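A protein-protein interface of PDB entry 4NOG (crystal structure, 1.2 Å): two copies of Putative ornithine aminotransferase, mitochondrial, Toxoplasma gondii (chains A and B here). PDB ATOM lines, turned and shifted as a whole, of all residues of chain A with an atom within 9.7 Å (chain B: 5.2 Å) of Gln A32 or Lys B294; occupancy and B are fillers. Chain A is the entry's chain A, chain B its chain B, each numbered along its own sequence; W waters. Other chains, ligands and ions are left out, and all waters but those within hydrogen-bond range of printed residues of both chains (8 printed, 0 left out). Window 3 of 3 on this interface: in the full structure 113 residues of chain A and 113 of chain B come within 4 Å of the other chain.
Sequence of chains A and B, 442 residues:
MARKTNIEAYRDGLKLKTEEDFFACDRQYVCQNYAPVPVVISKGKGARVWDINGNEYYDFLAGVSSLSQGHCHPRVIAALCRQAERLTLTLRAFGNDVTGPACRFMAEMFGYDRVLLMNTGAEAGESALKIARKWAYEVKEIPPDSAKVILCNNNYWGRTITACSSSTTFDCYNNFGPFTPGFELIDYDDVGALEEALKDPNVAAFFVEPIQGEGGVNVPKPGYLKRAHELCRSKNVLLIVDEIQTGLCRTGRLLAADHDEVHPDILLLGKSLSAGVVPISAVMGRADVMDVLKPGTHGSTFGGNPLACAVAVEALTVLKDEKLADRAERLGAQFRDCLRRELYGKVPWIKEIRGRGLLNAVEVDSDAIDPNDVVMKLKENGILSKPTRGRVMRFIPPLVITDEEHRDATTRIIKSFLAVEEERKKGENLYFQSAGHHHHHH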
ATOM      1  N   PHE A  23      17.111  17.906 -34.663  1.00  0.00           N
ATOM      2  CA  PHE A  23      17.322  16.774 -33.780  1.00  0.00           C
ATOM      3  C   PHE A  23      18.193  17.115 -32.570  1.00  0.00           C
ATOM      4  O   PHE A  23      17.930  16.657 -31.443  1.00  0.00           O
ATOM      5  CB  PHE A  23      17.943  15.571 -34.509  1.00  0.00           C
ATOM      6  CG  PHE A  23      17.167  15.033 -35.721  1.00  0.00           C
ATOM      7  CD1 PHE A  23      15.794  15.191 -35.839  1.00  0.00           C
ATOM      8  CD2 PHE A  23      17.846  14.320 -36.709  1.00  0.00           C
ATOM      9  CE1 PHE A  23      15.127  14.657 -36.922  1.00  0.00           C
ATOM     10  CE2 PHE A  23      17.158  13.804 -37.765  1.00  0.00           C
ATOM     11  CZ  PHE A  23      15.798  13.961 -37.877  1.00  0.00           C
ATOM     12  N   CYS A  25      18.520  20.054 -31.242  1.00  0.00           N
ATOM     13  CA  CYS A  25      17.718  20.933 -30.359  1.00  0.00           C
ATOM     14  C   CYS A  25      16.855  20.065 -29.417  1.00  0.00           C
ATOM     15  O   CYS A  25      16.786  20.303 -28.207  1.00  0.00           O
ATOM     16  CB  CYS A  25      16.918  21.900 -31.230  1.00  0.00           C
ATOM     17  SG  CYS A  25      15.841  23.061 -30.305  1.00  0.00           S
ATOM     18  N   ASP A  26      16.278  19.021 -29.950  1.00  0.00           N
ATOM     19  CA  ASP A  26      15.559  18.064 -29.055  1.00  0.00           C
ATOM     20  C   ASP A  26      16.424  17.516 -27.928  1.00  0.00           C
ATOM     21  O   ASP A  26      16.069  17.540 -26.760  1.00  0.00           O
ATOM     22  CB  ASP A  26      15.072  16.759 -29.775  1.00  0.00           C
ATOM     23  CG  ASP A  26      14.017  16.987 -30.677  1.00  0.00           C
ATOM     24  OD1 ASP A  26      13.301  17.978 -30.443  1.00  0.00           O
ATOM     25  OD2 ASP A  26      13.816  16.113 -31.577  1.00  0.00           O
ATOM     26  N   ARG A  27      17.502  16.815 -28.374  1.00  0.00           N
ATOM     27  CA  ARG A  27      18.452  16.239 -27.426  1.00  0.00           C
ATOM     28  C   ARG A  27      18.770  17.170 -26.286  1.00  0.00           C
ATOM     29  O   ARG A  27      18.946  16.685 -25.181  1.00  0.00           O
ATOM     30  CB  ARG A  27      19.767  15.693 -28.077  1.00  0.00           C
ATOM     31  CG  ARG A  27      19.585  14.514 -28.929  1.00  0.00           C
ATOM     32  CD  ARG A  27      20.876  13.898 -29.377  1.00  0.00           C
ATOM     33  NE  ARG A  27      21.489  14.713 -30.382  1.00  0.00           N
ATOM     34  CZ  ARG A  27      21.296  14.591 -31.697  1.00  0.00           C
ATOM     35  NH1 ARG A  27      20.492  13.694 -32.213  1.00  0.00           N
ATOM     36  NH2 ARG A  27      21.948  15.400 -32.479  1.00  0.00           N
ATOM     37  N   GLN A  28      18.940  18.442 -26.597  1.00  0.00           N
ATOM     38  CA  GLN A  28      19.382  19.365 -25.615  1.00  0.00           C
ATOM     39  C   GLN A  28      18.253  19.830 -24.718  1.00  0.00           C
ATOM     40  O   GLN A  28      18.514  19.966 -23.526  1.00  0.00           O
ATOM     41  CB  GLN A  28      20.097  20.547 -26.284  1.00  0.00           C
ATOM     42  CG  GLN A  28      20.777  21.486 -25.258  1.00  0.00           C
ATOM     43  CD  GLN A  28      21.815  20.823 -24.323  1.00  0.00           C
ATOM     44  OE1 GLN A  28      21.731  20.875 -23.107  1.00  0.00           O
ATOM     45  NE2 GLN A  28      22.805  20.241 -24.925  1.00  0.00           N
ATOM     46  N   TYR A  29      17.055  20.100 -25.266  1.00  0.00           N
ATOM     47  CA  TYR A  29      16.063  20.872 -24.491  1.00  0.00           C
ATOM     48  C   TYR A  29      14.769  20.126 -24.204  1.00  0.00           C
ATOM     49  O   TYR A  29      14.020  20.564 -23.330  1.00  0.00           O
ATOM     50  CB  TYR A  29      15.715  22.169 -25.236  1.00  0.00           C
ATOM     51  CG  TYR A  29      16.908  23.088 -25.354  1.00  0.00           C
ATOM     52  CD1 TYR A  29      17.435  23.782 -24.260  1.00  0.00           C
ATOM     53  CD2 TYR A  29      17.621  23.183 -26.589  1.00  0.00           C
ATOM     54  CE1 TYR A  29      18.583  24.568 -24.406  1.00  0.00           C
ATOM     55  CE2 TYR A  29      18.741  23.950 -26.692  1.00  0.00           C
ATOM     56  CZ  TYR A  29      19.216  24.664 -25.625  1.00  0.00           C
ATOM     57  OH  TYR A  29      20.345  25.416 -25.800  1.00  0.00           O
ATOM     58  N   VAL A  30      14.470  19.076 -24.928  1.00  0.00           N
ATOM     59  CA  VAL A  30      13.221  18.334 -24.857  1.00  0.00           C
ATOM     60  C   VAL A  30      13.432  17.101 -23.987  1.00  0.00           C
ATOM     61  O   VAL A  30      14.328  16.300 -24.245  1.00  0.00           O
ATOM     62  CB  VAL A  30      12.701  17.949 -26.224  1.00  0.00           C
ATOM     63  CG1 VAL A  30      11.356  17.295 -26.068  1.00  0.00           C
ATOM     64  CG2 VAL A  30      12.570  19.187 -27.080  1.00  0.00           C
ATOM     65  N   CYS A  31      12.581  16.872 -22.973  1.00  0.00           N
ATOM     66  CA  CYS A  31      12.645  15.666 -22.169  1.00  0.00           C
ATOM     67  C   CYS A  31      12.712  14.458 -23.110  1.00  0.00           C
ATOM     68  O   CYS A  31      11.920  14.372 -24.083  1.00  0.00           O
ATOM     69  CB  CYS A  31      11.408  15.592 -21.298  1.00  0.00           C
ATOM     70  SG  CYS A  31      11.376  14.190 -20.164  1.00  0.00           S
ATOM     71  N   GLN A  32      13.604  13.515 -22.848  1.00  0.00           N
ATOM     72  CA  GLN A  32      13.956  12.497 -23.889  1.00  0.00           C
ATOM     73  C   GLN A  32      13.165  11.228 -23.783  1.00  0.00           C
ATOM     74  O   GLN A  32      13.661  10.123 -23.917  1.00  0.00           O
ATOM     75  CB  GLN A  32      15.424  12.202 -23.785  1.00  0.00           C
ATOM     76  CG  GLN A  32      15.773  11.375 -22.527  1.00  0.00           C
ATOM     77  CD  GLN A  32      16.851  10.288 -22.641  1.00  0.00           C
ATOM     78  OE1 GLN A  32      17.010   9.567 -23.668  1.00  0.00           O
ATOM     79  NE2 GLN A  32      17.537  10.089 -21.514  1.00  0.00           N
ATOM     80  N   ASN A  33      11.845  11.373 -23.596  1.00  0.00           N
ATOM     81  CA  ASN A  33      10.980  10.225 -23.410  1.00  0.00           C
ATOM     82  C   ASN A  33      10.380   9.614 -24.690  1.00  0.00           C
ATOM     83  O   ASN A  33       9.577   8.709 -24.582  1.00  0.00           O
ATOM     84  CB  ASN A  33       9.897  10.520 -22.349  1.00  0.00           C
ATOM     85  CG  ASN A  33       8.982  11.626 -22.742  1.00  0.00           C
ATOM     86  OD1 ASN A  33       9.393  12.779 -22.844  1.00  0.00           O
ATOM     87  ND2 ASN A  33       7.706  11.323 -22.979  1.00  0.00           N
ATOM     88  N   TYR A  34      10.802  10.152 -25.839  1.00  0.00           N
ATOM     89  CA  TYR A  34      10.485   9.579 -27.123  1.00  0.00           C
ATOM     90  C   TYR A  34      11.768   9.181 -27.843  1.00  0.00           C
ATOM     91  O   TYR A  34      12.773   9.861 -27.750  1.00  0.00           O
ATOM     92  CB  TYR A  34       9.635  10.544 -27.970  1.00  0.00           C
ATOM     93  CG  TYR A  34       8.151  10.485 -27.645  1.00  0.00           C
ATOM     94  CD1 TYR A  34       7.649  11.203 -26.546  1.00  0.00           C
ATOM     95  CD2 TYR A  34       7.249   9.760 -28.424  1.00  0.00           C
ATOM     96  CE1 TYR A  34       6.288  11.164 -26.229  1.00  0.00           C
ATOM     97  CE2 TYR A  34       5.902   9.750 -28.096  1.00  0.00           C
ATOM     98  CZ  TYR A  34       5.423  10.411 -27.015  1.00  0.00           C
ATOM     99  OH  TYR A  34       4.102  10.386 -26.673  1.00  0.00           O
ATOM    100  N   ALA A  35      11.650   8.145 -28.641  1.00  0.00           N
ATOM    101  CA  ALA A  35      12.755   7.648 -29.419  1.00  0.00           C
ATOM    102  C   ALA A  35      13.124   8.687 -30.478  1.00  0.00           C
ATOM    103  O   ALA A  35      12.334   9.586 -30.840  1.00  0.00           O
ATOM    104  CB  ALA A  35      12.334   6.311 -30.054  1.00  0.00           C
ATOM    105  N   PRO A  36      14.352   8.592 -31.005  1.00  0.00           N
ATOM    106  CA  PRO A  36      14.650   9.433 -32.167  1.00  0.00           C
ATOM    107  C   PRO A  36      13.650   9.307 -33.315  1.00  0.00           C
ATOM    108  O   PRO A  36      12.942   8.305 -33.476  1.00  0.00           O
ATOM    109  CB  PRO A  36      16.036   8.903 -32.621  1.00  0.00           C
ATOM    110  CG  PRO A  36      16.661   8.306 -31.366  1.00  0.00           C
ATOM    111  CD  PRO A  36      15.486   7.693 -30.645  1.00  0.00           C
ATOM    112  N   ARG A 159      -0.951   7.369 -19.499  1.00  0.00           N
ATOM    113  CA  ARG A 159       0.334   7.428 -18.802  1.00  0.00           C
ATOM    114  C   ARG A 159       0.260   7.979 -17.399  1.00  0.00           C
ATOM    115  O   ARG A 159       1.332   8.174 -16.767  1.00  0.00           O
ATOM    116  CB  ARG A 159       1.342   8.193 -19.626  1.00  0.00           C
ATOM    117  CG  ARG A 159       1.617   7.594 -20.993  1.00  0.00           C
ATOM    118  CD  ARG A 159       2.443   6.341 -20.873  1.00  0.00           C
ATOM    119  NE  ARG A 159       2.923   5.947 -22.185  1.00  0.00           N
ATOM    120  CZ  ARG A 159       4.009   5.255 -22.403  1.00  0.00           C
ATOM    121  NH1 ARG A 159       4.798   4.841 -21.414  1.00  0.00           N
ATOM    122  NH2 ARG A 159       4.383   5.025 -23.628  1.00  0.00           N
ATOM    123  N   ASP A 171       7.851  -1.188 -19.795  1.00  0.00           N
ATOM    124  CA  ASP A 171       8.300   0.196 -19.763  1.00  0.00           C
ATOM    125  C   ASP A 171       7.254   1.177 -19.337  1.00  0.00           C
ATOM    126  O   ASP A 171       7.583   2.321 -18.937  1.00  0.00           O
ATOM    127  CB  ASP A 171       8.918   0.605 -21.062  1.00  0.00           C
ATOM    128  CG  ASP A 171      10.373   0.056 -21.193  1.00  0.00           C
ATOM    129  OD1 ASP A 171      11.112  -0.148 -20.157  1.00  0.00           O
ATOM    130  OD2 ASP A 171      10.819  -0.031 -22.315  1.00  0.00           O
ATOM    131  N   CYS A 172       5.965   0.827 -19.445  1.00  0.00           N
ATOM    132  CA  CYS A 172       4.922   1.708 -18.902  1.00  0.00           C
ATOM    133  C   CYS A 172       4.912   1.741 -17.386  1.00  0.00           C
ATOM    134  O   CYS A 172       4.588   2.778 -16.798  1.00  0.00           O
ATOM    135  CB  CYS A 172       3.531   1.306 -19.383  1.00  0.00           C
ATOM    136  SG  CYS A 172       3.265   1.645 -21.114  1.00  0.00           S
ATOM    137  N   ASN A 174       7.505   0.161 -15.096  1.00  0.00           N
ATOM    138  CA  ASN A 174       8.706  -0.086 -14.308  1.00  0.00           C
ATOM    139  C   ASN A 174       9.186   1.178 -13.605  1.00  0.00           C
ATOM    140  O   ASN A 174       9.385   2.220 -14.229  1.00  0.00           O
ATOM    141  CB  ASN A 174       9.757  -0.596 -15.259  1.00  0.00           C
ATOM    142  CG  ASN A 174      11.066  -0.896 -14.576  1.00  0.00           C
ATOM    143  OD1 ASN A 174      11.086  -1.601 -13.563  1.00  0.00           O
ATOM    144  ND2 ASN A 174      12.149  -0.290 -15.068  1.00  0.00           N
ATOM    145  N   ASN A 175       9.400   1.031 -12.308  1.00  0.00           N
ATOM    146  CA  ASN A 175       9.966   2.078 -11.477  1.00  0.00           C
ATOM    147  C   ASN A 175       9.056   3.280 -11.282  1.00  0.00           C
ATOM    148  O   ASN A 175       9.517   4.344 -10.892  1.00  0.00           O
ATOM    149  CB  ASN A 175      11.375   2.466 -11.902  1.00  0.00           C
ATOM    150  CG  ASN A 175      12.429   1.508 -11.373  1.00  0.00           C
ATOM    151  OD1 ASN A 175      12.179   0.763 -10.440  1.00  0.00           O
ATOM    152  ND2 ASN A 175      13.578   1.515 -11.989  1.00  0.00           N
ATOM    153  N   PHE A 176       7.740   3.092 -11.481  1.00  0.00           N
ATOM    154  CA  PHE A 176       6.792   4.174 -11.252  1.00  0.00           C
ATOM    155  C   PHE A 176       5.863   3.893 -10.080  1.00  0.00           C
ATOM    156  O   PHE A 176       4.947   4.689  -9.821  1.00  0.00           O
ATOM    157  CB  PHE A 176       5.997   4.488 -12.510  1.00  0.00           C
ATOM    158  CG  PHE A 176       6.780   5.024 -13.650  1.00  0.00           C
ATOM    159  CD1 PHE A 176       7.564   6.101 -13.528  1.00  0.00           C
ATOM    160  CD2 PHE A 176       6.639   4.454 -14.916  1.00  0.00           C
ATOM    161  CE1 PHE A 176       8.265   6.618 -14.594  1.00  0.00           C
ATOM    162  CE2 PHE A 176       7.316   4.944 -16.006  1.00  0.00           C
ATOM    163  CZ  PHE A 176       8.145   6.050 -15.850  1.00  0.00           C
ATOM    164  N   ARG B  92       4.863  13.127 -30.930  1.00  0.00           N
ATOM    165  CA  ARG B  92       6.296  13.135 -30.742  1.00  0.00           C
ATOM    166  C   ARG B  92       6.968  11.908 -31.379  1.00  0.00           C
ATOM    167  O   ARG B  92       8.185  11.795 -31.392  1.00  0.00           O
ATOM    168  CB  ARG B  92       6.615  13.277 -29.257  1.00  0.00           C
ATOM    169  CG  ARG B  92       6.371  14.727 -28.793  1.00  0.00           C
ATOM    170  CD  ARG B  92       6.753  14.961 -27.367  1.00  0.00           C
ATOM    171  NE  ARG B  92       8.191  14.766 -27.172  1.00  0.00           N
ATOM    172  CZ  ARG B  92       8.783  14.420 -26.036  1.00  0.00           C
ATOM    173  NH1 ARG B  92       8.119  14.464 -24.897  1.00  0.00           N
ATOM    174  NH2 ARG B  92      10.079  14.055 -26.072  1.00  0.00           N
ATOM    175  N   LYS B 134      10.914   7.418 -10.229  1.00  0.00           N
ATOM    176  CA  LYS B 134      11.903   6.702 -11.055  1.00  0.00           C
ATOM    177  C   LYS B 134      13.302   7.156 -10.700  1.00  0.00           C
ATOM    178  O   LYS B 134      14.235   6.355 -10.657  1.00  0.00           O
ATOM    179  CB  LYS B 134      11.564   6.892 -12.555  1.00  0.00           C
ATOM    180  CG  LYS B 134      12.360   6.002 -13.530  1.00  0.00           C
ATOM    181  CD  LYS B 134      11.912   6.195 -14.992  1.00  0.00           C
ATOM    182  CE  LYS B 134      12.204   5.024 -15.888  1.00  0.00           C
ATOM    183  NZ  LYS B 134      12.222   3.863 -14.969  1.00  0.00           N
ATOM    184  N   GLU B 138      16.318   4.787  -9.156  1.00  0.00           N
ATOM    185  CA  GLU B 138      17.485   4.611 -10.022  1.00  0.00           C
ATOM    186  C   GLU B 138      18.741   5.367  -9.552  1.00  0.00           C
ATOM    187  O   GLU B 138      19.844   4.909  -9.765  1.00  0.00           O
ATOM    188  CB  GLU B 138      17.173   5.002 -11.454  1.00  0.00           C
ATOM    189  CG  GLU B 138      16.130   4.059 -12.042  1.00  0.00           C
ATOM    190  CD  GLU B 138      15.680   4.333 -13.467  1.00  0.00           C
ATOM    191  OE1 GLU B 138      16.167   5.237 -14.095  1.00  0.00           O
ATOM    192  OE2 GLU B 138      14.819   3.567 -13.882  1.00  0.00           O
ATOM    193  N   ASP B 291      16.234  13.036 -17.186  1.00  0.00           N
ATOM    194  CA  ASP B 291      16.718  12.021 -18.127  1.00  0.00           C
ATOM    195  C   ASP B 291      16.379  10.611 -17.680  1.00  0.00           C
ATOM    196  O   ASP B 291      16.565   9.688 -18.493  1.00  0.00           O
ATOM    197  CB  ASP B 291      18.219  12.186 -18.394  1.00  0.00           C
ATOM    198  CG  ASP B 291      18.538  13.398 -19.285  1.00  0.00           C
ATOM    199  OD1 ASP B 291      17.596  14.097 -19.776  1.00  0.00           O
ATOM    200  OD2 ASP B 291      19.732  13.666 -19.439  1.00  0.00           O
ATOM    201  N   VAL B 292      15.791  10.414 -16.500  1.00  0.00           N
ATOM    202  CA  VAL B 292      15.299   9.071 -16.162  1.00  0.00           C
ATOM    203  C   VAL B 292      14.134   8.670 -17.029  1.00  0.00           C
ATOM    204  O   VAL B 292      13.776   7.492 -17.121  1.00  0.00           O
ATOM    205  CB  VAL B 292      14.908   8.950 -14.657  1.00  0.00           C
ATOM    206  CG1 VAL B 292      16.103   9.317 -13.775  1.00  0.00           C
ATOM    207  CG2 VAL B 292      13.625   9.714 -14.280  1.00  0.00           C
ATOM    208  N   LEU B 293      13.466   9.639 -17.630  1.00  0.00           N
ATOM    209  CA  LEU B 293      12.298   9.324 -18.465  1.00  0.00           C
ATOM    210  C   LEU B 293      12.762   8.948 -19.878  1.00  0.00           C
ATOM    211  O   LEU B 293      12.747   9.763 -20.779  1.00  0.00           O
ATOM    212  CB  LEU B 293      11.321  10.487 -18.520  1.00  0.00           C
ATOM    213  CG  LEU B 293      10.251  10.665 -17.529  1.00  0.00           C
ATOM    214  CD1 LEU B 293       9.190  11.613 -18.113  1.00  0.00           C
ATOM    215  CD2 LEU B 293       9.600   9.449 -16.955  1.00  0.00           C
ATOM    216  N   LYS B 294      13.183   7.697 -20.010  1.00  0.00           N
ATOM    217  CA  LYS B 294      13.766   7.160 -21.262  1.00  0.00           C
ATOM    218  C   LYS B 294      12.686   6.910 -22.300  1.00  0.00           C
ATOM    219  O   LYS B 294      11.507   6.819 -21.986  1.00  0.00           O
ATOM    220  CB  LYS B 294      14.453   5.854 -20.938  1.00  0.00           C
ATOM    221  CG  LYS B 294      15.592   6.038 -19.959  1.00  0.00           C
ATOM    222  CD  LYS B 294      16.758   6.703 -20.600  1.00  0.00           C
ATOM    223  CE  LYS B 294      18.003   6.583 -19.720  1.00  0.00           C
ATOM    224  NZ  LYS B 294      17.896   7.055 -18.301  1.00  0.00           N
ATOM    225  N   PRO B 295      13.095   6.672 -23.571  1.00  0.00           N
ATOM    226  CA  PRO B 295      12.096   6.453 -24.584  1.00  0.00           C
ATOM    227  C   PRO B 295      11.143   5.321 -24.237  1.00  0.00           C
ATOM    228  O   PRO B 295      11.567   4.237 -23.783  1.00  0.00           O
ATOM    229  CB  PRO B 295      12.958   6.152 -25.855  1.00  0.00           C
ATOM    230  CG  PRO B 295      14.161   6.975 -25.641  1.00  0.00           C
ATOM    231  CD  PRO B 295      14.439   6.921 -24.132  1.00  0.00           C
ATOM    232  N   GLY B 296       9.862   5.584 -24.470  1.00  0.00           N
ATOM    233  CA  GLY B 296       8.835   4.604 -24.212  1.00  0.00           C
ATOM    234  C   GLY B 296       8.313   4.536 -22.789  1.00  0.00           C
ATOM    235  O   GLY B 296       7.300   3.854 -22.562  1.00  0.00           O
ATOM    236  N   THR B 297       8.956   5.259 -21.863  1.00  0.00           N
ATOM    237  CA  THR B 297       8.517   5.220 -20.466  1.00  0.00           C
ATOM    238  C   THR B 297       7.485   6.242 -20.081  1.00  0.00           C
ATOM    239  O   THR B 297       7.034   6.244 -18.964  1.00  0.00           O
ATOM    240  CB  THR B 297       9.722   5.277 -19.477  1.00  0.00           C
ATOM    241  OG1 THR B 297      10.328   6.564 -19.509  1.00  0.00           O
ATOM    242  CG2 THR B 297      10.804   4.201 -19.830  1.00  0.00           C
ATOM    243  N   HIS B 298       7.188   7.132 -21.011  1.00  0.00           N
ATOM    244  CA  HIS B 298       6.171   8.167 -20.771  1.00  0.00           C
ATOM    245  C   HIS B 298       5.759   8.670 -22.116  1.00  0.00           C
ATOM    246  O   HIS B 298       6.476   8.529 -23.086  1.00  0.00           O
ATOM    247  CB  HIS B 298       6.745   9.297 -19.891  1.00  0.00           C
ATOM    248  CG  HIS B 298       5.715  10.211 -19.388  1.00  0.00           C
ATOM    249  ND1 HIS B 298       4.702   9.788 -18.551  1.00  0.00           N
ATOM    250  CD2 HIS B 298       5.541  11.532 -19.602  1.00  0.00           C
ATOM    251  CE1 HIS B 298       3.963  10.843 -18.248  1.00  0.00           C
ATOM    252  NE2 HIS B 298       4.462  11.903 -18.858  1.00  0.00           N
HETATM  253  O   HOH W   1       4.660   5.135 -18.369  1.00  0.00           O
HETATM  254  O   HOH W   2       5.840   1.389 -23.244  1.00  0.00           O
HETATM  255  O   HOH W   3       2.897  12.186 -29.052  1.00  0.00           O
HETATM  256  O   HOH W   4       7.582   7.169 -25.889  1.00  0.00           O
HETATM  257  O   HOH W   5      18.413  13.005 -22.854  1.00  0.00           O
HETATM  258  O   HOH W   6       9.623   2.649 -16.944  1.00  0.00           O
HETATM  259  O   HOH W   7      14.807  14.207 -20.257  1.00  0.00           O
HETATM  260  O   HOH W   8       9.675   9.275 -31.378  1.00  0.00           O
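Of the printed residues of chain B, Cys A31 touches Arg B92 and Leu B293.
Gln A32 touches just these residues of chain B: Asp B291 (3.2 Å), Leu B293 (3.3 Å), Lys B294 (3.6 Å) and Pro B295 (3.3 Å).
Printed residues of chain B within 4 Å of Ala A35: Pro B295.
Printed residues of chain B within 4 Å of Asp A171: Gly B296 and Thr B297.
Of the printed residues of chain A, Arg B92 touches Val A30 (3.5 Å), Cys A31 (2.7 Å), Asn A33 (2.9 Å) and Tyr A34 (3.4 Å).
Asp B291 touches just one residue of chain A: Gln A32.
Lys B294 touches two residues of chain A.
Gly B296 touches three residues of chain A.
Of the printed residues of chain A, His B298 touches Asn A33 and Arg A159.
The nearest residue of chain A that does not touch Lys B294 is Tyr A34 (5.1 Å).
The nearest printed residue of chain B that does not touch Ala A35 is Arg B92 (4.7 Å).
The side-chain amide nitrogen (ND2) of Asn A175 sits at hydrogen-bond distance from the side-chain carboxylate (OE2) of Glu B138 (3.1 Å).
O of Asn A175 sits close to N of Lys B134 (3.4 Å).
O of Gln A32 lies close to O of Leu B293 (3.3 Å).
N of Asn A33 sits close to O of Leu B293 (3.4 Å).
The side-chain amide nitrogen (ND2) of Asn A33 lies within hydrogen-bond range of the backbone carbonyl oxygen (O) of His B298 (3.1 Å).
The backbone NH of His B298 sits close to the guanidinium group of Arg A159, at 3.3 Å.
NE2 of Gln A32 lies within hydrogen-bond range of O of Asp B291 (3.2 Å).
The guanidinium group (NH2) of Arg B92 is in hydrogen-bond range of the backbone carbonyl oxygen (O) of Cys A31 (2.7 Å).
The side-chain amino group (NZ) of Lys B134 sits at hydrogen-bond distance from the backbone carbonyl oxygen (O) of Asn A174, at 3.4 Å.
The backbone carbonyl oxygen (O) of Asn A33 is in hydrogen-bond range of the backbone NH (N) of Gly B296 (3.1 Å).
NH1 of Arg A159 lies within hydrogen-bond range of O of Gly B296 (2.9 Å).
The side-chain amide oxygen of Asn A33 sits at hydrogen-bond distance from the guanidinium group of Arg B92, at 2.9 Å.
No position is printed for both chains.
NH2 of Arg B92 touches CG1 of Val A30, 3.5 Å away.
Leu B293 touches Cys A31 (CD1 to SG, 3.95 Å).
CD of Lys B294 touches NE2 of Gln A32, at 3.6 Å.
Pro B295 touches Gln A32.
Asn A33 touches Pro B295 (O to CA, 3.4 Å).
Arg B92 touches Tyr A34.
Arg A159 touches Thr B297.
Lys B134 touches Phe A176.
Phe A176 touches Leu B293 (CZ to CD2, 3.9 Å).
Phe A176 touches Thr B297.
O of Cys A31 lies close to OD1 of Asn A33.
OE2 of Glu B138 lies within salt-bridge range of NZ of Lys B134 (2.8 Å).
The side-chain sulfur of Cys A172 lies within hydrogen-bond range of the guanidinium group of Arg A159 (3.6 Å).
O of Asp B291 sits at hydrogen-bond distance from NZ of Lys B294, at 3.0 Å.
O of Lys B294 lies within hydrogen-bond range of OG1 of Thr B297 (2.8 Å).
Hydrophobic or aromatic side chains of chain B that line the printed part of chain A: Leu B293, Pro B295 and His B298.
Printed residues of chain A that touch a printed residue of chain B: Val A30, Cys A31, Gln A32, Asn A33, Tyr A34, Ala A35, Arg A159, Asp A171, Asn A174, Asn A175 and Phe A176.
Hydrophobic or aromatic side chains of chain A within 4 Å of the printed part of chain B: Val A30, Tyr A34 and Phe A176.
Among the printed residues, 27 pairs touch across the chains.
Water W1 lies within hydrogen-bond range of the backbone carbonyl oxygen (O) of Thr B297 (2.7 Å), the backbone carbonyl oxygen (O) of Cys A172 (2.8 Å) and the guanidinium group (NH1) of Arg A159 (3.1 Å).
Water W8 lies within hydrogen-bond range of O of Ala A35 and O of Arg B92.
Water W6 lies within hydrogen-bond range of O of Asn A174 (2.8 Å), O of Asp A171 (2.9 Å) and NZ of Lys B134 (3.5 Å).
Water W7 lies within hydrogen-bond range of OD1 of Asp B291, N of Gln A32 and SG of Cys A31.
Water W4 lies within hydrogen-bond range of the backbone carbonyl oxygen of Asn A33 (2.8 Å), the backbone NH of Gly B296 (3.1 Å) and the backbone carbonyl oxygen of His B298 (3.3 Å).
Water W2 lies within hydrogen-bond range of the backbone carbonyl oxygen of Gly B296 and the side-chain sulfur of Cys A172.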
